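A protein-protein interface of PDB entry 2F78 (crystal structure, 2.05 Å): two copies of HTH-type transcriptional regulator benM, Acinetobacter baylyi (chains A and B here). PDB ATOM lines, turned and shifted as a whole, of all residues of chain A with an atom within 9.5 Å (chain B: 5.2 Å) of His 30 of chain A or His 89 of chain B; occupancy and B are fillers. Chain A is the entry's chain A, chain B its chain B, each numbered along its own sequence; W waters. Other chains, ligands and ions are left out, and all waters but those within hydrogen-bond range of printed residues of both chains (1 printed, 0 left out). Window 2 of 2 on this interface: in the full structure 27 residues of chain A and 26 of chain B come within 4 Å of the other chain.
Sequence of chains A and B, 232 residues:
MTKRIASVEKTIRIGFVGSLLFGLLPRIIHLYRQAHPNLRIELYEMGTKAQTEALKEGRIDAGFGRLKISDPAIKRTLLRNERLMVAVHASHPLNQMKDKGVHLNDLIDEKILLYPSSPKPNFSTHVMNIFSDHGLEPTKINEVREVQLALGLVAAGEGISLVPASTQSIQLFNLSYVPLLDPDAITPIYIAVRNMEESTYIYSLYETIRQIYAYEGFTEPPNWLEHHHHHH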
ATOM      1  N   ILE A  14       3.603 -31.988   8.907  1.00  0.00           N
ATOM      2  CA  ILE A  14       3.224 -30.633   9.260  1.00  0.00           C
ATOM      3  C   ILE A  14       3.254 -29.740   8.046  1.00  0.00           C
ATOM      4  O   ILE A  14       4.287 -29.599   7.387  1.00  0.00           O
ATOM      5  CB  ILE A  14       4.130 -30.059  10.394  1.00  0.00           C
ATOM      6  CG1 ILE A  14       3.903 -30.850  11.690  1.00  0.00           C
ATOM      7  CG2 ILE A  14       3.832 -28.573  10.629  1.00  0.00           C
ATOM      8  CD1 ILE A  14       4.967 -30.660  12.749  1.00  0.00           C
ATOM      9  N   LEU A  24       8.866 -18.388  14.755  1.00  0.00           N
ATOM     10  CA  LEU A  24       9.147 -19.396  15.780  1.00  0.00           C
ATOM     11  C   LEU A  24       9.043 -20.825  15.306  1.00  0.00           C
ATOM     12  O   LEU A  24       9.357 -21.729  16.068  1.00  0.00           O
ATOM     13  CB  LEU A  24       8.205 -19.220  16.978  1.00  0.00           C
ATOM     14  CG  LEU A  24       8.236 -17.870  17.694  1.00  0.00           C
ATOM     15  CD1 LEU A  24       7.159 -17.809  18.753  1.00  0.00           C
ATOM     16  CD2 LEU A  24       9.597 -17.598  18.314  1.00  0.00           C
ATOM     17  N   LEU A  25       8.617 -21.045  14.063  1.00  0.00           N
ATOM     18  CA  LEU A  25       8.411 -22.399  13.565  1.00  0.00           C
ATOM     19  C   LEU A  25       9.619 -23.321  13.718  1.00  0.00           C
ATOM     20  O   LEU A  25       9.483 -24.420  14.259  1.00  0.00           O
ATOM     21  CB  LEU A  25       7.926 -22.401  12.100  1.00  0.00           C
ATOM     22  CG  LEU A  25       7.588 -23.787  11.519  1.00  0.00           C
ATOM     23  CD1 LEU A  25       6.545 -24.506  12.364  1.00  0.00           C
ATOM     24  CD2 LEU A  25       7.132 -23.669  10.066  1.00  0.00           C
ATOM     25  N   PRO A  26      10.795 -22.910  13.214  1.00  0.00           N
ATOM     26  CA  PRO A  26      11.948 -23.807  13.356  1.00  0.00           C
ATOM     27  C   PRO A  26      12.328 -24.192  14.796  1.00  0.00           C
ATOM     28  O   PRO A  26      12.658 -25.353  15.030  1.00  0.00           O
ATOM     29  CB  PRO A  26      13.079 -23.029  12.671  1.00  0.00           C
ATOM     30  CG  PRO A  26      12.371 -22.144  11.687  1.00  0.00           C
ATOM     31  CD  PRO A  26      11.150 -21.697  12.459  1.00  0.00           C
ATOM     32  N   ARG A  27      12.299 -23.262  15.752  1.00  0.00           N
ATOM     33  CA  ARG A  27      12.661 -23.599  17.138  1.00  0.00           C
ATOM     34  C   ARG A  27      11.593 -24.484  17.791  1.00  0.00           C
ATOM     35  O   ARG A  27      11.908 -25.328  18.628  1.00  0.00           O
ATOM     36  CB  ARG A  27      12.949 -22.340  17.978  1.00  0.00           C
ATOM     37  CG  ARG A  27      11.760 -21.719  18.690  1.00  0.00           C
ATOM     38  CD  ARG A  27      12.168 -20.528  19.542  1.00  0.00           C
ATOM     39  NE  ARG A  27      12.652 -19.388  18.760  1.00  0.00           N
ATOM     40  CZ  ARG A  27      12.808 -18.154  19.237  1.00  0.00           C
ATOM     41  NH1 ARG A  27      12.516 -17.873  20.502  1.00  0.00           N
ATOM     42  NH2 ARG A  27      13.251 -17.189  18.445  1.00  0.00           N
ATOM     43  N   ILE A  28      10.338 -24.286  17.397  1.00  0.00           N
ATOM     44  CA  ILE A  28       9.239 -25.127  17.850  1.00  0.00           C
ATOM     45  C   ILE A  28       9.395 -26.569  17.338  1.00  0.00           C
ATOM     46  O   ILE A  28       9.281 -27.519  18.102  1.00  0.00           O
ATOM     47  CB  ILE A  28       7.870 -24.542  17.429  1.00  0.00           C
ATOM     48  CG1 ILE A  28       7.553 -23.295  18.258  1.00  0.00           C
ATOM     49  CG2 ILE A  28       6.760 -25.566  17.617  1.00  0.00           C
ATOM     50  CD1 ILE A  28       6.373 -22.467  17.719  1.00  0.00           C
ATOM     51  N   ILE A  29       9.682 -26.721  16.055  1.00  0.00           N
ATOM     52  CA  ILE A  29       9.907 -28.040  15.467  1.00  0.00           C
ATOM     53  C   ILE A  29      11.166 -28.690  16.037  1.00  0.00           C
ATOM     54  O   ILE A  29      11.163 -29.890  16.334  1.00  0.00           O
ATOM     55  CB  ILE A  29      10.004 -27.948  13.917  1.00  0.00           C
ATOM     56  CG1 ILE A  29       8.633 -27.589  13.317  1.00  0.00           C
ATOM     57  CG2 ILE A  29      10.581 -29.230  13.325  1.00  0.00           C
ATOM     58  CD1 ILE A  29       7.466 -28.418  13.816  1.00  0.00           C
ATOM     59  N   HIS A  30      12.235 -27.915  16.204  1.00  0.00           N
ATOM     60  CA  HIS A  30      13.467 -28.469  16.775  1.00  0.00           C
ATOM     61  C   HIS A  30      13.274 -29.017  18.194  1.00  0.00           C
ATOM     62  O   HIS A  30      13.789 -30.082  18.531  1.00  0.00           O
ATOM     63  CB  HIS A  30      14.576 -27.426  16.796  1.00  0.00           C
ATOM     64  CG  HIS A  30      15.914 -27.986  17.156  1.00  0.00           C
ATOM     65  ND1 HIS A  30      16.389 -27.996  18.447  1.00  0.00           N
ATOM     66  CD2 HIS A  30      16.883 -28.543  16.396  1.00  0.00           C
ATOM     67  CE1 HIS A  30      17.588 -28.550  18.472  1.00  0.00           C
ATOM     68  NE2 HIS A  30      17.914 -28.885  17.236  1.00  0.00           N
ATOM     69  N   LEU A  31      12.567 -28.267  19.030  1.00  0.00           N
ATOM     70  CA  LEU A  31      12.287 -28.698  20.405  1.00  0.00           C
ATOM     71  C   LEU A  31      11.329 -29.903  20.445  1.00  0.00           C
ATOM     72  O   LEU A  31      11.512 -30.839  21.230  1.00  0.00           O
ATOM     73  CB  LEU A  31      11.719 -27.525  21.218  1.00  0.00           C
ATOM     74  CG  LEU A  31      11.317 -27.824  22.668  1.00  0.00           C
ATOM     75  CD1 LEU A  31      12.471 -28.462  23.440  1.00  0.00           C
ATOM     76  CD2 LEU A  31      10.828 -26.565  23.359  1.00  0.00           C
ATOM     77  N   TYR A  32      10.311 -29.867  19.595  1.00  0.00           N
ATOM     78  CA  TYR A  32       9.348 -30.964  19.458  1.00  0.00           C
ATOM     79  C   TYR A  32      10.060 -32.279  19.094  1.00  0.00           C
ATOM     80  O   TYR A  32       9.803 -33.323  19.705  1.00  0.00           O
ATOM     81  CB  TYR A  32       8.297 -30.571  18.403  1.00  0.00           C
ATOM     82  CG  TYR A  32       7.201 -31.584  18.164  1.00  0.00           C
ATOM     83  CD1 TYR A  32       6.395 -32.038  19.205  1.00  0.00           C
ATOM     84  CD2 TYR A  32       6.946 -32.068  16.883  1.00  0.00           C
ATOM     85  CE1 TYR A  32       5.384 -32.959  18.979  1.00  0.00           C
ATOM     86  CE2 TYR A  32       5.934 -32.992  16.649  1.00  0.00           C
ATOM     87  CZ  TYR A  32       5.160 -33.434  17.701  1.00  0.00           C
ATOM     88  OH  TYR A  32       4.161 -34.350  17.466  1.00  0.00           O
ATOM     89  N   ARG A  33      10.955 -32.215  18.102  1.00  0.00           N
ATOM     90  CA  ARG A  33      11.778 -33.362  17.692  1.00  0.00           C
ATOM     91  C   ARG A  33      12.673 -33.868  18.817  1.00  0.00           C
ATOM     92  O   ARG A  33      12.815 -35.062  19.020  1.00  0.00           O
ATOM     93  CB  ARG A  33      12.699 -32.986  16.527  1.00  0.00           C
ATOM     94  CG  ARG A  33      12.037 -32.951  15.181  1.00  0.00           C
ATOM     95  CD  ARG A  33      13.015 -32.449  14.135  1.00  0.00           C
ATOM     96  NE  ARG A  33      12.534 -32.739  12.791  1.00  0.00           N
ATOM     97  CZ  ARG A  33      12.775 -31.992  11.720  1.00  0.00           C
ATOM     98  NH1 ARG A  33      13.498 -30.889  11.820  1.00  0.00           N
ATOM     99  NH2 ARG A  33      12.290 -32.356  10.545  1.00  0.00           N
ATOM    100  N   GLN A  34      13.309 -32.933  19.511  1.00  0.00           N
ATOM    101  CA  GLN A  34      14.226 -33.245  20.591  1.00  0.00           C
ATOM    102  C   GLN A  34      13.513 -33.954  21.736  1.00  0.00           C
ATOM    103  O   GLN A  34      13.996 -34.964  22.249  1.00  0.00           O
ATOM    104  CB  GLN A  34      14.858 -31.948  21.077  1.00  0.00           C
ATOM    105  CG  GLN A  34      15.842 -32.080  22.201  1.00  0.00           C
ATOM    106  CD  GLN A  34      16.547 -30.758  22.472  1.00  0.00           C
ATOM    107  OE1 GLN A  34      17.385 -30.322  21.686  1.00  0.00           O
ATOM    108  NE2 GLN A  34      16.190 -30.107  23.575  1.00  0.00           N
ATOM    109  N   ALA A  35      12.354 -33.435  22.131  1.00  0.00           N
ATOM    110  CA  ALA A  35      11.589 -34.022  23.238  1.00  0.00           C
ATOM    111  C   ALA A  35      10.896 -35.333  22.866  1.00  0.00           C
ATOM    112  O   ALA A  35      10.456 -36.073  23.752  1.00  0.00           O
ATOM    113  CB  ALA A  35      10.583 -33.028  23.764  1.00  0.00           C
ATOM    114  N   HIS A  36      10.812 -35.622  21.565  1.00  0.00           N
ATOM    115  CA  HIS A  36      10.083 -36.782  21.064  1.00  0.00           C
ATOM    116  C   HIS A  36      10.903 -37.519  20.009  1.00  0.00           C
ATOM    117  O   HIS A  36      10.514 -37.567  18.846  1.00  0.00           O
ATOM    118  CB  HIS A  36       8.732 -36.331  20.494  1.00  0.00           C
ATOM    119  CG  HIS A  36       7.910 -35.550  21.471  1.00  0.00           C
ATOM    120  ND1 HIS A  36       7.132 -36.157  22.432  1.00  0.00           N
ATOM    121  CD2 HIS A  36       7.791 -34.216  21.676  1.00  0.00           C
ATOM    122  CE1 HIS A  36       6.547 -35.229  23.171  1.00  0.00           C
ATOM    123  NE2 HIS A  36       6.927 -34.044  22.730  1.00  0.00           N
ATOM    124  N   PRO A  37      12.037 -38.114  20.421  1.00  0.00           N
ATOM    125  CA  PRO A  37      12.978 -38.743  19.489  1.00  0.00           C
ATOM    126  C   PRO A  37      12.421 -40.009  18.818  1.00  0.00           C
ATOM    127  O   PRO A  37      13.009 -40.498  17.851  1.00  0.00           O
ATOM    128  CB  PRO A  37      14.177 -39.077  20.379  1.00  0.00           C
ATOM    129  CG  PRO A  37      13.624 -39.200  21.729  1.00  0.00           C
ATOM    130  CD  PRO A  37      12.477 -38.262  21.822  1.00  0.00           C
ATOM    131  N   LEU A  39       9.526 -39.922  17.348  1.00  0.00           N
ATOM    132  CA  LEU A  39       8.735 -39.412  16.233  1.00  0.00           C
ATOM    133  C   LEU A  39       9.606 -38.946  15.082  1.00  0.00           C
ATOM    134  O   LEU A  39      10.681 -38.377  15.291  1.00  0.00           O
ATOM    135  CB  LEU A  39       7.880 -38.225  16.686  1.00  0.00           C
ATOM    136  CG  LEU A  39       6.975 -38.451  17.893  1.00  0.00           C
ATOM    137  CD1 LEU A  39       6.238 -37.160  18.216  1.00  0.00           C
ATOM    138  CD2 LEU A  39       5.986 -39.594  17.641  1.00  0.00           C
ATOM    139  N   ILE A  41       9.247 -36.269  12.124  1.00  0.00           N
ATOM    140  CA  ILE A  41       8.455 -35.111  11.722  1.00  0.00           C
ATOM    141  C   ILE A  41       8.855 -34.695  10.307  1.00  0.00           C
ATOM    142  O   ILE A  41      10.041 -34.575  10.018  1.00  0.00           O
ATOM    143  CB  ILE A  41       8.620 -33.930  12.719  1.00  0.00           C
ATOM    144  CG1 ILE A  41       7.972 -34.278  14.071  1.00  0.00           C
ATOM    145  CG2 ILE A  41       7.979 -32.657  12.173  1.00  0.00           C
ATOM    146  CD1 ILE A  41       8.753 -35.257  14.909  1.00  0.00           C
ATOM    147  N   LEU A  43       8.072 -31.814   7.193  1.00  0.00           N
ATOM    148  CA  LEU A  43       7.580 -30.457   6.978  1.00  0.00           C
ATOM    149  C   LEU A  43       7.262 -30.227   5.510  1.00  0.00           C
ATOM    150  O   LEU A  43       8.078 -30.524   4.627  1.00  0.00           O
ATOM    151  CB  LEU A  43       8.612 -29.427   7.448  1.00  0.00           C
ATOM    152  CG  LEU A  43       9.005 -29.527   8.927  1.00  0.00           C
ATOM    153  CD1 LEU A  43      10.122 -28.564   9.256  1.00  0.00           C
ATOM    154  CD2 LEU A  43       7.807 -29.263   9.817  1.00  0.00           C
ATOM    155  N   LEU A 205       2.622 -31.430  20.386  1.00  0.00           N
ATOM    156  CA  LEU A 205       2.984 -30.255  19.604  1.00  0.00           C
ATOM    157  C   LEU A 205       2.380 -28.996  20.225  1.00  0.00           C
ATOM    158  O   LEU A 205       3.062 -27.988  20.346  1.00  0.00           O
ATOM    159  CB  LEU A 205       2.538 -30.410  18.152  1.00  0.00           C
ATOM    160  CG  LEU A 205       2.779 -29.217  17.224  1.00  0.00           C
ATOM    161  CD1 LEU A 205       4.279 -28.941  17.088  1.00  0.00           C
ATOM    162  CD2 LEU A 205       2.136 -29.484  15.882  1.00  0.00           C
ATOM    163  N   THR A 208       4.541 -27.952  23.165  1.00  0.00           N
ATOM    164  CA  THR A 208       5.788 -27.336  22.718  1.00  0.00           C
ATOM    165  C   THR A 208       5.573 -25.869  22.380  1.00  0.00           C
ATOM    166  O   THR A 208       6.382 -25.028  22.740  1.00  0.00           O
ATOM    167  CB  THR A 208       6.358 -28.065  21.486  1.00  0.00           C
ATOM    168  OG1 THR A 208       6.534 -29.447  21.797  1.00  0.00           O
ATOM    169  CG2 THR A 208       7.682 -27.477  21.063  1.00  0.00           C
ATOM    170  N   ILE A 212       7.294 -22.552  24.323  1.00  0.00           N
ATOM    171  CA  ILE A 212       7.978 -21.457  23.613  1.00  0.00           C
ATOM    172  C   ILE A 212       7.253 -20.123  23.820  1.00  0.00           C
ATOM    173  O   ILE A 212       7.881 -19.090  24.061  1.00  0.00           O
ATOM    174  CB  ILE A 212       8.104 -21.753  22.082  1.00  0.00           C
ATOM    175  CG1 ILE A 212       8.958 -23.001  21.835  1.00  0.00           C
ATOM    176  CG2 ILE A 212       8.692 -20.555  21.328  1.00  0.00           C
ATOM    177  CD1 ILE A 212      10.353 -22.932  22.420  1.00  0.00           C
ATOM    178  N   ALA B  87      25.478 -23.528   6.137  1.00  0.00           N
ATOM    179  CA  ALA B  87      24.465 -23.204   7.119  1.00  0.00           C
ATOM    180  C   ALA B  87      24.204 -24.447   7.956  1.00  0.00           C
ATOM    181  O   ALA B  87      23.875 -25.517   7.410  1.00  0.00           O
ATOM    182  CB  ALA B  87      23.190 -22.755   6.419  1.00  0.00           C
ATOM    183  N   VAL B  88      24.372 -24.312   9.269  1.00  0.00           N
ATOM    184  CA  VAL B  88      24.227 -25.433  10.197  1.00  0.00           C
ATOM    185  C   VAL B  88      23.417 -25.013  11.420  1.00  0.00           C
ATOM    186  O   VAL B  88      23.280 -23.826  11.694  1.00  0.00           O
ATOM    187  CB  VAL B  88      25.606 -25.975  10.674  1.00  0.00           C
ATOM    188  CG1 VAL B  88      26.446 -26.427   9.475  1.00  0.00           C
ATOM    189  CG2 VAL B  88      26.363 -24.941  11.524  1.00  0.00           C
ATOM    190  N   HIS B  89      22.888 -25.985  12.158  1.00  0.00           N
ATOM    191  CA  HIS B  89      22.281 -25.666  13.444  1.00  0.00           C
ATOM    192  C   HIS B  89      23.404 -25.354  14.426  1.00  0.00           C
ATOM    193  O   HIS B  89      24.491 -25.950  14.349  1.00  0.00           O
ATOM    194  CB  HIS B  89      21.432 -26.821  13.980  1.00  0.00           C
ATOM    195  CG  HIS B  89      20.550 -26.427  15.124  1.00  0.00           C
ATOM    196  ND1 HIS B  89      20.865 -26.701  16.437  1.00  0.00           N
ATOM    197  CD2 HIS B  89      19.383 -25.740  15.153  1.00  0.00           C
ATOM    198  CE1 HIS B  89      19.926 -26.210  17.225  1.00  0.00           C
ATOM    199  NE2 HIS B  89      19.013 -25.625  16.471  1.00  0.00           N
ATOM    200  N   ALA B  90      23.137 -24.432  15.345  1.00  0.00           N
ATOM    201  CA  ALA B  90      24.095 -24.045  16.392  1.00  0.00           C
ATOM    202  C   ALA B  90      24.793 -25.240  17.044  1.00  0.00           C
ATOM    203  O   ALA B  90      25.973 -25.191  17.341  1.00  0.00           O
ATOM    204  CB  ALA B  90      23.390 -23.209  17.454  1.00  0.00           C
ATOM    205  N   SER B  91      24.051 -26.320  17.244  1.00  0.00           N
ATOM    206  CA  SER B  91      24.544 -27.516  17.952  1.00  0.00           C
ATOM    207  C   SER B  91      25.364 -28.472  17.085  1.00  0.00           C
ATOM    208  O   SER B  91      25.932 -29.430  17.597  1.00  0.00           O
ATOM    209  CB  SER B  91      23.356 -28.307  18.493  1.00  0.00           C
ATOM    210  OG  SER B  91      22.631 -28.862  17.405  1.00  0.00           O
ATOM    211  N   HIS B  92      25.406 -28.233  15.781  1.00  0.00           N
ATOM    212  CA  HIS B  92      26.019 -29.176  14.852  1.00  0.00           C
ATOM    213  C   HIS B  92      27.535 -29.240  15.052  1.00  0.00           C
ATOM    214  O   HIS B  92      28.156 -28.207  15.262  1.00  0.00           O
ATOM    215  CB  HIS B  92      25.696 -28.792  13.403  1.00  0.00           C
ATOM    216  CG  HIS B  92      25.958 -29.895  12.430  1.00  0.00           C
ATOM    217  ND1 HIS B  92      24.998 -30.817  12.074  1.00  0.00           N
ATOM    218  CD2 HIS B  92      27.082 -30.254  11.774  1.00  0.00           C
ATOM    219  CE1 HIS B  92      25.520 -31.688  11.232  1.00  0.00           C
ATOM    220  NE2 HIS B  92      26.785 -31.372  11.037  1.00  0.00           N
ATOM    221  N   ASN B  95      29.811 -26.755  13.443  1.00  0.00           N
ATOM    222  CA  ASN B  95      29.822 -25.413  14.021  1.00  0.00           C
ATOM    223  C   ASN B  95      30.934 -25.222  15.057  1.00  0.00           C
ATOM    224  O   ASN B  95      31.184 -24.104  15.487  1.00  0.00           O
ATOM    225  CB  ASN B  95      28.455 -25.056  14.627  1.00  0.00           C
ATOM    226  CG  ASN B  95      28.210 -23.560  14.685  1.00  0.00           C
ATOM    227  OD1 ASN B  95      28.665 -22.795  13.825  1.00  0.00           O
ATOM    228  ND2 ASN B  95      27.456 -23.139  15.674  1.00  0.00           N
ATOM    229  N   VAL B 154      17.099 -26.291   8.030  1.00  0.00           N
ATOM    230  CA  VAL B 154      18.325 -26.442   8.820  1.00  0.00           C
ATOM    231  C   VAL B 154      18.077 -26.039  10.283  1.00  0.00           C
ATOM    232  O   VAL B 154      18.409 -26.778  11.218  1.00  0.00           O
ATOM    233  CB  VAL B 154      19.520 -25.627   8.224  1.00  0.00           C
ATOM    234  CG1 VAL B 154      20.730 -25.702   9.135  1.00  0.00           C
ATOM    235  CG2 VAL B 154      19.904 -26.139   6.836  1.00  0.00           C
ATOM    236  N   ALA B 155      17.484 -24.866  10.470  1.00  0.00           N
ATOM    237  CA  ALA B 155      17.205 -24.338  11.796  1.00  0.00           C
ATOM    238  C   ALA B 155      16.238 -25.224  12.590  1.00  0.00           C
ATOM    239  O   ALA B 155      16.318 -25.277  13.808  1.00  0.00           O
ATOM    240  CB  ALA B 155      16.670 -22.910  11.687  1.00  0.00           C
ATOM    241  N   ALA B 156      15.336 -25.914  11.891  1.00  0.00           N
ATOM    242  CA  ALA B 156      14.393 -26.853  12.515  1.00  0.00           C
ATOM    243  C   ALA B 156      15.061 -28.172  12.902  1.00  0.00           C
ATOM    244  O   ALA B 156      14.494 -28.961  13.657  1.00  0.00           O
ATOM    245  CB  ALA B 156      13.209 -27.102  11.600  1.00  0.00           C
ATOM    246  N   GLY B 157      16.264 -28.408  12.385  1.00  0.00           N
ATOM    247  CA  GLY B 157      17.110 -29.492  12.878  1.00  0.00           C
ATOM    248  C   GLY B 157      17.239 -30.717  11.994  1.00  0.00           C
ATOM    249  O   GLY B 157      17.575 -31.794  12.479  1.00  0.00           O
ATOM    250  N   GLY B 159      19.310 -31.198   8.521  1.00  0.00           N
ATOM    251  CA  GLY B 159      20.107 -30.896   7.344  1.00  0.00           C
ATOM    252  C   GLY B 159      21.116 -29.784   7.521  1.00  0.00           C
ATOM    253  O   GLY B 159      21.157 -29.115   8.559  1.00  0.00           O
ATOM    254  N   ASN B 174      19.282 -19.845  16.215  1.00  0.00           N
ATOM    255  CA  ASN B 174      20.138 -21.046  16.255  1.00  0.00           C
ATOM    256  C   ASN B 174      20.640 -21.543  14.894  1.00  0.00           C
ATOM    257  O   ASN B 174      21.006 -22.718  14.738  1.00  0.00           O
ATOM    258  CB  ASN B 174      19.443 -22.185  17.017  1.00  0.00           C
ATOM    259  CG  ASN B 174      19.812 -22.220  18.471  1.00  0.00           C
ATOM    260  OD1 ASN B 174      20.854 -21.703  18.867  1.00  0.00           O
ATOM    261  ND2 ASN B 174      18.961 -22.836  19.286  1.00  0.00           N
ATOM    262  N   LEU B 175      20.677 -20.630  13.932  1.00  0.00           N
ATOM    263  CA  LEU B 175      21.291 -20.866  12.636  1.00  0.00           C
ATOM    264  C   LEU B 175      22.656 -20.197  12.630  1.00  0.00           C
ATOM    265  O   LEU B 175      22.801 -19.037  13.018  1.00  0.00           O
ATOM    266  CB  LEU B 175      20.413 -20.303  11.520  1.00  0.00           C
ATOM    267  CG  LEU B 175      20.901 -20.445  10.076  1.00  0.00           C
ATOM    268  CD1 LEU B 175      20.749 -21.877   9.597  1.00  0.00           C
ATOM    269  CD2 LEU B 175      20.128 -19.474   9.165  1.00  0.00           C
ATOM    270  N   SER B 176      23.657 -20.946  12.191  1.00  0.00           N
ATOM    271  CA  SER B 176      25.030 -20.483  12.183  1.00  0.00           C
ATOM    272  C   SER B 176      25.636 -20.777  10.819  1.00  0.00           C
ATOM    273  O   SER B 176      25.314 -21.789  10.214  1.00  0.00           O
ATOM    274  CB  SER B 176      25.803 -21.203  13.284  1.00  0.00           C
ATOM    275  OG  SER B 176      27.161 -20.801  13.307  1.00  0.00           O
HETATM  276  O   HOH W   1      20.484 -29.927  19.349  1.00  0.00           O
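The guanidinium group (NH1) of Arg 33 of chain A sits at hydrogen-bond distance from the backbone carbonyl oxygen (O) of Ala 156 of chain B, 2.8 Å away.
A ring nitrogen (ND1) of His 89 of chain B lies within hydrogen-bond range of the side-chain hydroxyl (OG) of Ser 91 of chain B (3.0 Å). NH2 of Arg 33 of chain A sits at hydrogen-bond distance from O of Ile 41 of chain A.
Pro 26 of chain A touches Ala 155 of chain B (CB to CB, 3.7 Å). Pro 26 of chain A touches Ala 156 of chain B. CB of Ala 156 of chain B touches CG2 of Ile 29 of chain A, 3.8 Å away. CE1 of His 89 of chain B touches NE2 of His 30 of chain A, at 3.3 Å. Ala 156 of chain B touches His 30 of chain A. His 30 of chain A touches Gly 157 of chain B. C of Gly 157 of chain B touches NH1 of Arg 33 of chain A, at 3.7 Å.
Of chain B, only His 89 (3.3 Å), Ala 156 (3.3 Å) and Gly 157 (3.7 Å) come within 4 Å of His 30 of chain A. No residue of chain A comes within 4 Å of Val 88 of chain B. No residue of chain A comes within 4 Å of Ser 91 of chain B. Of the printed residues of chain A, Ala 155 of chain B touches Pro 26. Of chain A, only His 30 and Arg 33 come within 4 Å of Gly 157 of chain B. Printed residues of chain B within 4 Å of Ile 29 of chain A: Ala 156 (3.8 Å). Of the printed residues of chain B, Arg 33 of chain A touches Ala 156 and Gly 157. Of the printed residues of chain B, Pro 26 of chain A touches Ala 155 (3.7 Å) and Ala 156 (3.4 Å). The nearest residue of chain A that does not touch His 89 of chain B is Pro 26 of chain A (6.5 Å).
Of the 15 printed residues of chain B, 4 touch a printed residue of chain A. Hydrophobic or aromatic side chains of chain B within 4 Å of the printed part of chain A: His 89, Ala 155 and Ala 156. Hydrophobic or aromatic side chains of chain A that line the printed part of chain B: Pro 26, Ile 29 and His 30. Among the printed residues, 8 pairs touch across the chains. Among the printed residues, no Asp or Glu carboxylate lies within 4 Å of a Lys or Arg side-chain nitrogen of the other chain.
No position is printed for both chains.
Water W1 bridges the side-chain hydroxyl (OG) of Ser 91 of chain B (3.1 Å) and a ring nitrogen (NE2) of His 30 of chain A (3.5 Å).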
